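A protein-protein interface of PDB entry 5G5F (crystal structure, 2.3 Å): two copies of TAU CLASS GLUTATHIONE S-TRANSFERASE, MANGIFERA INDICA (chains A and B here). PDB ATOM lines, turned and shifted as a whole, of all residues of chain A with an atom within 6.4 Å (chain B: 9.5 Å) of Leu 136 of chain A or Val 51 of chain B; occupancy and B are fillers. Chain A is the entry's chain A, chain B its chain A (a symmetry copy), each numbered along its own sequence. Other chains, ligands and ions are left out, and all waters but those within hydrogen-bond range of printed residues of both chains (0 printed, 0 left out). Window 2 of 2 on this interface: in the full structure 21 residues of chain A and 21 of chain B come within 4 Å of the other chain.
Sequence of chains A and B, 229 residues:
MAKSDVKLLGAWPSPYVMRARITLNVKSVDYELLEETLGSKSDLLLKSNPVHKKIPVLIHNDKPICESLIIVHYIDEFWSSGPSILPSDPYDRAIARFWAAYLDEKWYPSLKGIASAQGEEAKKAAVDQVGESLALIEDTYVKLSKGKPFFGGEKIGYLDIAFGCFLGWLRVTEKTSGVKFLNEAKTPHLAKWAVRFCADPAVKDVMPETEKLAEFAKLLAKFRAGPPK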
ATOM      1  N   PHE A  98       9.218   8.752  21.070  1.00  0.00           N
ATOM      2  CA  PHE A  98       9.885   9.952  21.563  1.00  0.00           C
ATOM      3  C   PHE A  98      10.555  10.731  20.439  1.00  0.00           C
ATOM      4  O   PHE A  98      10.400  11.948  20.338  1.00  0.00           O
ATOM      5  CB  PHE A  98      10.921   9.598  22.632  1.00  0.00           C
ATOM      6  CG  PHE A  98      11.826  10.742  22.997  1.00  0.00           C
ATOM      7  CD1 PHE A  98      11.383  11.754  23.834  1.00  0.00           C
ATOM      8  CD2 PHE A  98      13.119  10.809  22.501  1.00  0.00           C
ATOM      9  CE1 PHE A  98      12.210  12.810  24.170  1.00  0.00           C
ATOM     10  CE2 PHE A  98      13.951  11.863  22.834  1.00  0.00           C
ATOM     11  CZ  PHE A  98      13.495  12.864  23.669  1.00  0.00           C
ATOM     12  N   TRP A  99      11.302  10.028  19.597  1.00  0.00           N
ATOM     13  CA  TRP A  99      12.050  10.680  18.532  1.00  0.00           C
ATOM     14  C   TRP A  99      11.138  11.174  17.418  1.00  0.00           C
ATOM     15  O   TRP A  99      11.425  12.185  16.783  1.00  0.00           O
ATOM     16  CB  TRP A  99      13.118   9.737  17.977  1.00  0.00           C
ATOM     17  CG  TRP A  99      14.260   9.573  18.920  1.00  0.00           C
ATOM     18  CD1 TRP A  99      14.583   8.459  19.634  1.00  0.00           C
ATOM     19  CD2 TRP A  99      15.218  10.575  19.282  1.00  0.00           C
ATOM     20  NE1 TRP A  99      15.694   8.698  20.407  1.00  0.00           N
ATOM     21  CE2 TRP A  99      16.101   9.991  20.209  1.00  0.00           C
ATOM     22  CE3 TRP A  99      15.417  11.906  18.904  1.00  0.00           C
ATOM     23  CZ2 TRP A  99      17.169  10.694  20.765  1.00  0.00           C
ATOM     24  CZ3 TRP A  99      16.476  12.601  19.456  1.00  0.00           C
ATOM     25  CH2 TRP A  99      17.338  11.994  20.376  1.00  0.00           C
ATOM     26  N   TYR A 102       9.840  14.214  18.818  1.00  0.00           N
ATOM     27  CA  TYR A 102      10.955  15.154  18.816  1.00  0.00           C
ATOM     28  C   TYR A 102      11.108  15.832  17.461  1.00  0.00           C
ATOM     29  O   TYR A 102      11.363  17.033  17.381  1.00  0.00           O
ATOM     30  CB  TYR A 102      12.255  14.442  19.193  1.00  0.00           C
ATOM     31  CG  TYR A 102      13.502  15.228  18.855  1.00  0.00           C
ATOM     32  CD1 TYR A 102      13.912  16.288  19.650  1.00  0.00           C
ATOM     33  CD2 TYR A 102      14.273  14.907  17.745  1.00  0.00           C
ATOM     34  CE1 TYR A 102      15.050  17.009  19.351  1.00  0.00           C
ATOM     35  CE2 TYR A 102      15.415  15.623  17.436  1.00  0.00           C
ATOM     36  CZ  TYR A 102      15.798  16.673  18.244  1.00  0.00           C
ATOM     37  OH  TYR A 102      16.932  17.393  17.947  1.00  0.00           O
ATOM     38  N   LYS A 106      10.527  19.754  17.619  1.00  0.00           N
ATOM     39  CA  LYS A 106      11.798  20.469  17.608  1.00  0.00           C
ATOM     40  C   LYS A 106      12.480  20.530  16.242  1.00  0.00           C
ATOM     41  O   LYS A 106      12.752  21.617  15.733  1.00  0.00           O
ATOM     42  CB  LYS A 106      12.758  19.843  18.623  1.00  0.00           C
ATOM     43  CG  LYS A 106      12.568  20.342  20.045  1.00  0.00           C
ATOM     44  CD  LYS A 106      13.688  21.292  20.442  1.00  0.00           C
ATOM     45  CE  LYS A 106      13.406  21.958  21.777  1.00  0.00           C
ATOM     46  NZ  LYS A 106      13.334  20.970  22.888  1.00  0.00           N
ATOM     47  N   GLY A 131      22.247  20.802  12.348  1.00  0.00           N
ATOM     48  CA  GLY A 131      23.420  19.947  12.323  1.00  0.00           C
ATOM     49  C   GLY A 131      23.551  19.123  13.590  1.00  0.00           C
ATOM     50  O   GLY A 131      23.847  17.930  13.534  1.00  0.00           O
ATOM     51  N   GLU A 132      23.327  19.763  14.734  1.00  0.00           N
ATOM     52  CA  GLU A 132      23.398  19.082  16.024  1.00  0.00           C
ATOM     53  C   GLU A 132      22.329  18.003  16.144  1.00  0.00           C
ATOM     54  O   GLU A 132      22.608  16.886  16.579  1.00  0.00           O
ATOM     55  CB  GLU A 132      23.252  20.084  17.173  1.00  0.00           C
ATOM     56  CG  GLU A 132      24.396  21.079  17.297  1.00  0.00           C
ATOM     57  CD  GLU A 132      25.649  20.468  17.899  1.00  0.00           C
ATOM     58  OE1 GLU A 132      25.627  19.268  18.249  1.00  0.00           O
ATOM     59  OE2 GLU A 132      26.659  21.192  18.026  1.00  0.00           O
ATOM     60  N   SER A 133      21.106  18.350  15.758  1.00  0.00           N
ATOM     61  CA  SER A 133      19.988  17.419  15.816  1.00  0.00           C
ATOM     62  C   SER A 133      20.243  16.185  14.956  1.00  0.00           C
ATOM     63  O   SER A 133      19.935  15.066  15.360  1.00  0.00           O
ATOM     64  CB  SER A 133      18.699  18.110  15.372  1.00  0.00           C
ATOM     65  OG  SER A 133      18.059  18.750  16.461  1.00  0.00           O
ATOM     66  N   LEU A 134      20.815  16.395  13.775  1.00  0.00           N
ATOM     67  CA  LEU A 134      21.107  15.291  12.869  1.00  0.00           C
ATOM     68  C   LEU A 134      22.174  14.375  13.456  1.00  0.00           C
ATOM     69  O   LEU A 134      22.175  13.169  13.209  1.00  0.00           O
ATOM     70  CB  LEU A 134      21.551  15.812  11.502  1.00  0.00           C
ATOM     71  CG  LEU A 134      20.872  15.133  10.313  1.00  0.00           C
ATOM     72  CD1 LEU A 134      19.419  15.571  10.205  1.00  0.00           C
ATOM     73  CD2 LEU A 134      21.619  15.417   9.024  1.00  0.00           C
ATOM     74  N   ALA A 135      23.084  14.956  14.232  1.00  0.00           N
ATOM     75  CA  ALA A 135      24.091  14.177  14.942  1.00  0.00           C
ATOM     76  C   ALA A 135      23.422  13.340  16.024  1.00  0.00           C
ATOM     77  O   ALA A 135      23.786  12.185  16.248  1.00  0.00           O
ATOM     78  CB  ALA A 135      25.147  15.087  15.543  1.00  0.00           C
ATOM     79  N   LEU A 136      22.437  13.934  16.687  1.00  0.00           N
ATOM     80  CA  LEU A 136      21.651  13.242  17.702  1.00  0.00           C
ATOM     81  C   LEU A 136      20.855  12.103  17.075  1.00  0.00           C
ATOM     82  O   LEU A 136      20.676  11.047  17.681  1.00  0.00           O
ATOM     83  CB  LEU A 136      20.711  14.221  18.408  1.00  0.00           C
ATOM     84  CG  LEU A 136      20.400  13.963  19.882  1.00  0.00           C
ATOM     85  CD1 LEU A 136      21.682  13.833  20.688  1.00  0.00           C
ATOM     86  CD2 LEU A 136      19.522  15.072  20.440  1.00  0.00           C
ATOM     87  N   ILE A 137      20.382  12.328  15.853  1.00  0.00           N
ATOM     88  CA  ILE A 137      19.602  11.336  15.122  1.00  0.00           C
ATOM     89  C   ILE A 137      20.513  10.253  14.542  1.00  0.00           C
ATOM     90  O   ILE A 137      20.144   9.078  14.497  1.00  0.00           O
ATOM     91  CB  ILE A 137      18.777  12.000  13.995  1.00  0.00           C
ATOM     92  CG1 ILE A 137      17.728  12.940  14.591  1.00  0.00           C
ATOM     93  CG2 ILE A 137      18.094  10.955  13.128  1.00  0.00           C
ATOM     94  CD1 ILE A 137      17.236  13.995  13.627  1.00  0.00           C
ATOM     95  N   GLU A 138      21.707  10.655  14.113  1.00  0.00           N
ATOM     96  CA  GLU A 138      22.704   9.718  13.605  1.00  0.00           C
ATOM     97  C   GLU A 138      23.037   8.643  14.637  1.00  0.00           C
ATOM     98  O   GLU A 138      23.013   7.452  14.333  1.00  0.00           O
ATOM     99  CB  GLU A 138      23.979  10.462  13.195  1.00  0.00           C
ATOM    100  CG  GLU A 138      25.191   9.565  12.966  1.00  0.00           C
ATOM    101  CD  GLU A 138      25.184   8.876  11.612  1.00  0.00           C
ATOM    102  OE1 GLU A 138      24.232   9.084  10.832  1.00  0.00           O
ATOM    103  OE2 GLU A 138      26.139   8.124  11.326  1.00  0.00           O
ATOM    104  N   ASP A 139      23.337   9.071  15.859  1.00  0.00           N
ATOM    105  CA  ASP A 139      23.689   8.139  16.923  1.00  0.00           C
ATOM    106  C   ASP A 139      22.457   7.395  17.428  1.00  0.00           C
ATOM    107  O   ASP A 139      22.556   6.264  17.904  1.00  0.00           O
ATOM    108  CB  ASP A 139      24.379   8.871  18.075  1.00  0.00           C
ATOM    109  CG  ASP A 139      25.460   8.033  18.730  1.00  0.00           C
ATOM    110  OD1 ASP A 139      26.101   7.230  18.019  1.00  0.00           O
ATOM    111  OD2 ASP A 139      25.671   8.179  19.953  1.00  0.00           O
ATOM    112  N   THR A 140      21.298   8.037  17.325  1.00  0.00           N
ATOM    113  CA  THR A 140      20.032   7.390  17.650  1.00  0.00           C
ATOM    114  C   THR A 140      19.803   6.215  16.709  1.00  0.00           C
ATOM    115  O   THR A 140      19.377   5.138  17.129  1.00  0.00           O
ATOM    116  CB  THR A 140      18.845   8.367  17.551  1.00  0.00           C
ATOM    117  OG1 THR A 140      19.015   9.426  18.502  1.00  0.00           O
ATOM    118  CG2 THR A 140      17.531   7.649  17.825  1.00  0.00           C
ATOM    119  N   TYR A 141      20.098   6.433  15.431  1.00  0.00           N
ATOM    120  CA  TYR A 141      19.988   5.386  14.426  1.00  0.00           C
ATOM    121  C   TYR A 141      20.913   4.216  14.741  1.00  0.00           C
ATOM    122  O   TYR A 141      20.498   3.060  14.688  1.00  0.00           O
ATOM    123  CB  TYR A 141      20.304   5.937  13.033  1.00  0.00           C
ATOM    124  CG  TYR A 141      20.403   4.864  11.972  1.00  0.00           C
ATOM    125  CD1 TYR A 141      19.262   4.336  11.385  1.00  0.00           C
ATOM    126  CD2 TYR A 141      21.638   4.376  11.562  1.00  0.00           C
ATOM    127  CE1 TYR A 141      19.345   3.351  10.418  1.00  0.00           C
ATOM    128  CE2 TYR A 141      21.732   3.391  10.596  1.00  0.00           C
ATOM    129  CZ  TYR A 141      20.583   2.883  10.028  1.00  0.00           C
ATOM    130  OH  TYR A 141      20.671   1.903   9.066  1.00  0.00           O
ATOM    131  N   LYS B  41      17.255  23.228  37.278  1.00  0.00           N
ATOM    132  CA  LYS B  41      17.077  21.854  36.827  1.00  0.00           C
ATOM    133  C   LYS B  41      18.155  20.938  37.390  1.00  0.00           C
ATOM    134  O   LYS B  41      19.348  21.217  37.270  1.00  0.00           O
ATOM    135  CB  LYS B  41      17.067  21.793  35.299  1.00  0.00           C
ATOM    136  CG  LYS B  41      15.851  22.463  34.679  1.00  0.00           C
ATOM    137  CD  LYS B  41      15.774  22.232  33.182  1.00  0.00           C
ATOM    138  CE  LYS B  41      14.521  22.868  32.602  1.00  0.00           C
ATOM    139  NZ  LYS B  41      14.829  24.016  31.708  1.00  0.00           N
ATOM    140  N   LEU B  45      17.866  15.230  35.997  1.00  0.00           N
ATOM    141  CA  LEU B  45      16.916  15.603  34.954  1.00  0.00           C
ATOM    142  C   LEU B  45      17.653  15.940  33.662  1.00  0.00           C
ATOM    143  O   LEU B  45      17.169  15.659  32.564  1.00  0.00           O
ATOM    144  CB  LEU B  45      16.059  16.791  35.401  1.00  0.00           C
ATOM    145  CG  LEU B  45      15.157  17.429  34.341  1.00  0.00           C
ATOM    146  CD1 LEU B  45      14.144  16.421  33.820  1.00  0.00           C
ATOM    147  CD2 LEU B  45      14.455  18.663  34.890  1.00  0.00           C
ATOM    148  N   LEU B  46      18.830  16.539  33.807  1.00  0.00           N
ATOM    149  CA  LEU B  46      19.659  16.905  32.665  1.00  0.00           C
ATOM    150  C   LEU B  46      20.245  15.666  31.992  1.00  0.00           C
ATOM    151  O   LEU B  46      20.263  15.571  30.765  1.00  0.00           O
ATOM    152  CB  LEU B  46      20.774  17.858  33.099  1.00  0.00           C
ATOM    153  CG  LEU B  46      20.320  19.287  33.413  1.00  0.00           C
ATOM    154  CD1 LEU B  46      21.380  20.044  34.198  1.00  0.00           C
ATOM    155  CD2 LEU B  46      19.968  20.026  32.133  1.00  0.00           C
ATOM    156  N   LYS B  47      20.725  14.722  32.797  1.00  0.00           N
ATOM    157  CA  LYS B  47      21.209  13.448  32.272  1.00  0.00           C
ATOM    158  C   LYS B  47      20.073  12.641  31.651  1.00  0.00           C
ATOM    159  O   LYS B  47      20.225  12.061  30.576  1.00  0.00           O
ATOM    160  CB  LYS B  47      21.874  12.611  33.372  1.00  0.00           C
ATOM    161  CG  LYS B  47      23.190  13.143  33.916  1.00  0.00           C
ATOM    162  CD  LYS B  47      23.737  12.188  34.976  1.00  0.00           C
ATOM    163  CE  LYS B  47      25.048  12.677  35.567  1.00  0.00           C
ATOM    164  NZ  LYS B  47      24.900  14.002  36.229  1.00  0.00           N
ATOM    165  N   SER B  48      18.937  12.605  32.342  1.00  0.00           N
ATOM    166  CA  SER B  48      17.824  11.742  31.958  1.00  0.00           C
ATOM    167  C   SER B  48      17.018  12.297  30.792  1.00  0.00           C
ATOM    168  O   SER B  48      16.404  11.539  30.050  1.00  0.00           O
ATOM    169  CB  SER B  48      16.897  11.506  33.151  1.00  0.00           C
ATOM    170  OG  SER B  48      17.596  10.899  34.223  1.00  0.00           O
ATOM    171  N   ASN B  49      17.003  13.616  30.646  1.00  0.00           N
ATOM    172  CA  ASN B  49      16.307  14.242  29.528  1.00  0.00           C
ATOM    173  C   ASN B  49      17.111  15.410  28.970  1.00  0.00           C
ATOM    174  O   ASN B  49      16.759  16.565  29.183  1.00  0.00           O
ATOM    175  CB  ASN B  49      14.913  14.710  29.958  1.00  0.00           C
ATOM    176  CG  ASN B  49      14.044  15.129  28.782  1.00  0.00           C
ATOM    177  OD1 ASN B  49      14.440  15.003  27.623  1.00  0.00           O
ATOM    178  ND2 ASN B  49      12.849  15.627  29.079  1.00  0.00           N
ATOM    179  N   PRO B  50      18.203  15.110  28.254  1.00  0.00           N
ATOM    180  CA  PRO B  50      19.059  16.165  27.701  1.00  0.00           C
ATOM    181  C   PRO B  50      18.389  16.916  26.554  1.00  0.00           C
ATOM    182  O   PRO B  50      18.699  18.083  26.311  1.00  0.00           O
ATOM    183  CB  PRO B  50      20.283  15.394  27.203  1.00  0.00           C
ATOM    184  CG  PRO B  50      19.761  14.033  26.893  1.00  0.00           C
ATOM    185  CD  PRO B  50      18.695  13.763  27.915  1.00  0.00           C
ATOM    186  N   VAL B  51      17.472  16.245  25.867  1.00  0.00           N
ATOM    187  CA  VAL B  51      16.827  16.799  24.684  1.00  0.00           C
ATOM    188  C   VAL B  51      15.836  17.914  25.016  1.00  0.00           C
ATOM    189  O   VAL B  51      15.921  19.013  24.468  1.00  0.00           O
ATOM    190  CB  VAL B  51      16.094  15.698  23.893  1.00  0.00           C
ATOM    191  CG1 VAL B  51      15.179  16.310  22.850  1.00  0.00           C
ATOM    192  CG2 VAL B  51      17.098  14.749  23.251  1.00  0.00           C
ATOM    193  N   HIS B  52      14.899  17.629  25.914  1.00  0.00           N
ATOM    194  CA  HIS B  52      13.854  18.589  26.257  1.00  0.00           C
ATOM    195  C   HIS B  52      14.096  19.253  27.605  1.00  0.00           C
ATOM    196  O   HIS B  52      13.633  20.369  27.843  1.00  0.00           O
ATOM    197  CB  HIS B  52      12.484  17.907  26.264  1.00  0.00           C
ATOM    198  CG  HIS B  52      12.017  17.479  24.909  1.00  0.00           C
ATOM    199  ND1 HIS B  52      11.600  16.192  24.639  1.00  0.00           N
ATOM    200  CD2 HIS B  52      11.891  18.166  23.750  1.00  0.00           C
ATOM    201  CE1 HIS B  52      11.245  16.104  23.371  1.00  0.00           C
ATOM    202  NE2 HIS B  52      11.409  17.289  22.808  1.00  0.00           N
ATOM    203  N   LYS B  53      14.820  18.556  28.478  1.00  0.00           N
ATOM    204  CA  LYS B  53      15.050  19.004  29.850  1.00  0.00           C
ATOM    205  C   LYS B  53      13.722  19.247  30.556  1.00  0.00           C
ATOM    206  O   LYS B  53      13.572  20.199  31.317  1.00  0.00           O
ATOM    207  CB  LYS B  53      15.923  20.263  29.871  1.00  0.00           C
ATOM    208  CG  LYS B  53      17.298  20.055  29.253  1.00  0.00           C
ATOM    209  CD  LYS B  53      18.123  21.332  29.260  1.00  0.00           C
ATOM    210  CE  LYS B  53      19.493  21.101  28.638  1.00  0.00           C
ATOM    211  NZ  LYS B  53      20.432  22.224  28.911  1.00  0.00           N
ATOM    212  N   LYS B  54      12.762  18.366  30.295  1.00  0.00           N
ATOM    213  CA  LYS B  54      11.425  18.495  30.860  1.00  0.00           C
ATOM    214  C   LYS B  54      11.040  17.315  31.745  1.00  0.00           C
ATOM    215  O   LYS B  54      11.477  16.184  31.530  1.00  0.00           O
ATOM    216  CB  LYS B  54      10.387  18.647  29.746  1.00  0.00           C
ATOM    217  CG  LYS B  54      10.485  19.938  28.958  1.00  0.00           C
ATOM    218  CD  LYS B  54       9.319  20.067  27.991  1.00  0.00           C
ATOM    219  CE  LYS B  54       9.335  21.406  27.278  1.00  0.00           C
ATOM    220  NZ  LYS B  54       8.149  22.233  27.637  1.00  0.00           N
ATOM    221  N   VAL B  57       9.984  12.495  33.884  1.00  0.00           N
ATOM    222  CA  VAL B  57      10.831  11.453  33.323  1.00  0.00           C
ATOM    223  C   VAL B  57      10.681  10.189  34.156  1.00  0.00           C
ATOM    224  O   VAL B  57      10.972  10.189  35.353  1.00  0.00           O
ATOM    225  CB  VAL B  57      12.315  11.863  33.278  1.00  0.00           C
ATOM    226  CG1 VAL B  57      13.156  10.735  32.695  1.00  0.00           C
ATOM    227  CG2 VAL B  57      12.493  13.138  32.468  1.00  0.00           C
ATOM    228  N   PRO B  64      15.626   5.933  30.896  1.00  0.00           N
ATOM    229  CA  PRO B  64      14.694   7.065  30.874  1.00  0.00           C
ATOM    230  C   PRO B  64      13.564   6.895  29.862  1.00  0.00           C
ATOM    231  O   PRO B  64      13.788   6.411  28.754  1.00  0.00           O
ATOM    232  CB  PRO B  64      15.586   8.254  30.485  1.00  0.00           C
ATOM    233  CG  PRO B  64      17.001   7.771  30.642  1.00  0.00           C
ATOM    234  CD  PRO B  64      16.950   6.304  30.374  1.00  0.00           C
ATOM    235  N   CYS B  66      10.655   9.554  28.381  1.00  0.00           N
ATOM    236  CA  CYS B  66      10.239  10.952  28.426  1.00  0.00           C
ATOM    237  C   CYS B  66       8.889  11.183  27.754  1.00  0.00           C
ATOM    238  O   CYS B  66       8.378  10.308  27.052  1.00  0.00           O
ATOM    239  CB  CYS B  66      11.306  11.838  27.778  1.00  0.00           C
ATOM    240  SG  CYS B  66      12.945  11.695  28.534  1.00  0.00           S
ATOM    241  N   GLU B  67       8.335  12.375  27.983  1.00  0.00           N
ATOM    242  CA  GLU B  67       6.998  12.771  27.526  1.00  0.00           C
ATOM    243  C   GLU B  67       5.909  11.963  28.228  1.00  0.00           C
ATOM    244  O   GLU B  67       5.847  10.739  28.106  1.00  0.00           O
ATOM    245  CB  GLU B  67       6.872  12.640  26.005  1.00  0.00           C
ATOM    246  CG  GLU B  67       7.809  13.551  25.232  1.00  0.00           C
ATOM    247  CD  GLU B  67       7.466  15.019  25.407  1.00  0.00           C
ATOM    248  OE1 GLU B  67       6.261  15.345  25.456  1.00  0.00           O
ATOM    249  OE2 GLU B  67       8.399  15.845  25.490  1.00  0.00           O
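OE2 of Glu 67 of chain B is in hydrogen-bond range of ND1 of His 52 of chain B (3.3 Å).
OD1 of Asn 49 of chain B lies within hydrogen-bond range of N of His 52 of chain B.
The backbone carbonyl oxygen (O) of Ser 48 of chain B sits at hydrogen-bond distance from the side-chain sulfur (SG) of Cys 66 of chain B, at 3.8 Å.
The backbone carbonyl oxygen (O) of Leu 136 of chain A is in hydrogen-bond range of the side-chain hydroxyl (OG1) of Thr 140 of chain A, 2.5 Å away.
OD1 of Asn 49 of chain B lies close to SG of Cys 66 of chain B, at 3.7 Å.
Among the printed residues, pairs that only touch across the chains: Lys 106 of chain A with His 52 of chain B, Tyr 102 of chain A with Val 51 of chain B, Phe 98 of chain A with His 52 of chain B, Lys 106 of chain A with Val 51 of chain B, Leu 136 of chain A with Val 51 of chain B, Phe 98 of chain A with Cys 66 of chain B, Phe 98 of chain A with Val 51 of chain B and Trp 99 of chain A with Val 51 of chain B.
Printed residues of chain B within 4 Å of Trp 99 of chain A: Val 51.
Of the printed residues of chain B, Tyr 102 of chain A touches Val 51.
Printed residues of chain B within 4 Å of Lys 106 of chain A: Val 51 (3.6 Å) and His 52 (3.3 Å).
No residue of chain B comes within 4 Å of Ala 135 of chain A.
Leu 136 of chain A touches just one residue of chain B: Val 51 (3.7 Å).
Lys 41 of chain B touches none of the printed residues of chain A.
Printed residues of chain A within 4 Å of Val 51 of chain B: Phe 98, Trp 99, Tyr 102, Lys 106 and Leu 136.
Printed residues of chain A within 4 Å of His 52 of chain B: Phe 98 (3.5 Å) and Lys 106 (3.3 Å).
Pro 64 of chain B touches none of the printed residues of chain A.
Of the printed residues of chain A, Cys 66 of chain B touches Phe 98 (3.8 Å).
Of the 15 printed residues of chain A, 5 touch a printed residue of chain B.
Hydrophobic or aromatic side chains of chain A that line the printed part of chain B: Phe 98, Trp 99, Tyr 102 and Leu 136.
Of the 15 printed residues of chain B, 3 touch a printed residue of chain A.
Among the printed residues, 8 pairs touch across the chains.
Among the printed residues, no Asp or Glu carboxylate lies within 4 Å of a Lys or Arg side-chain nitrogen of the other chain.
No position is printed for both chains.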
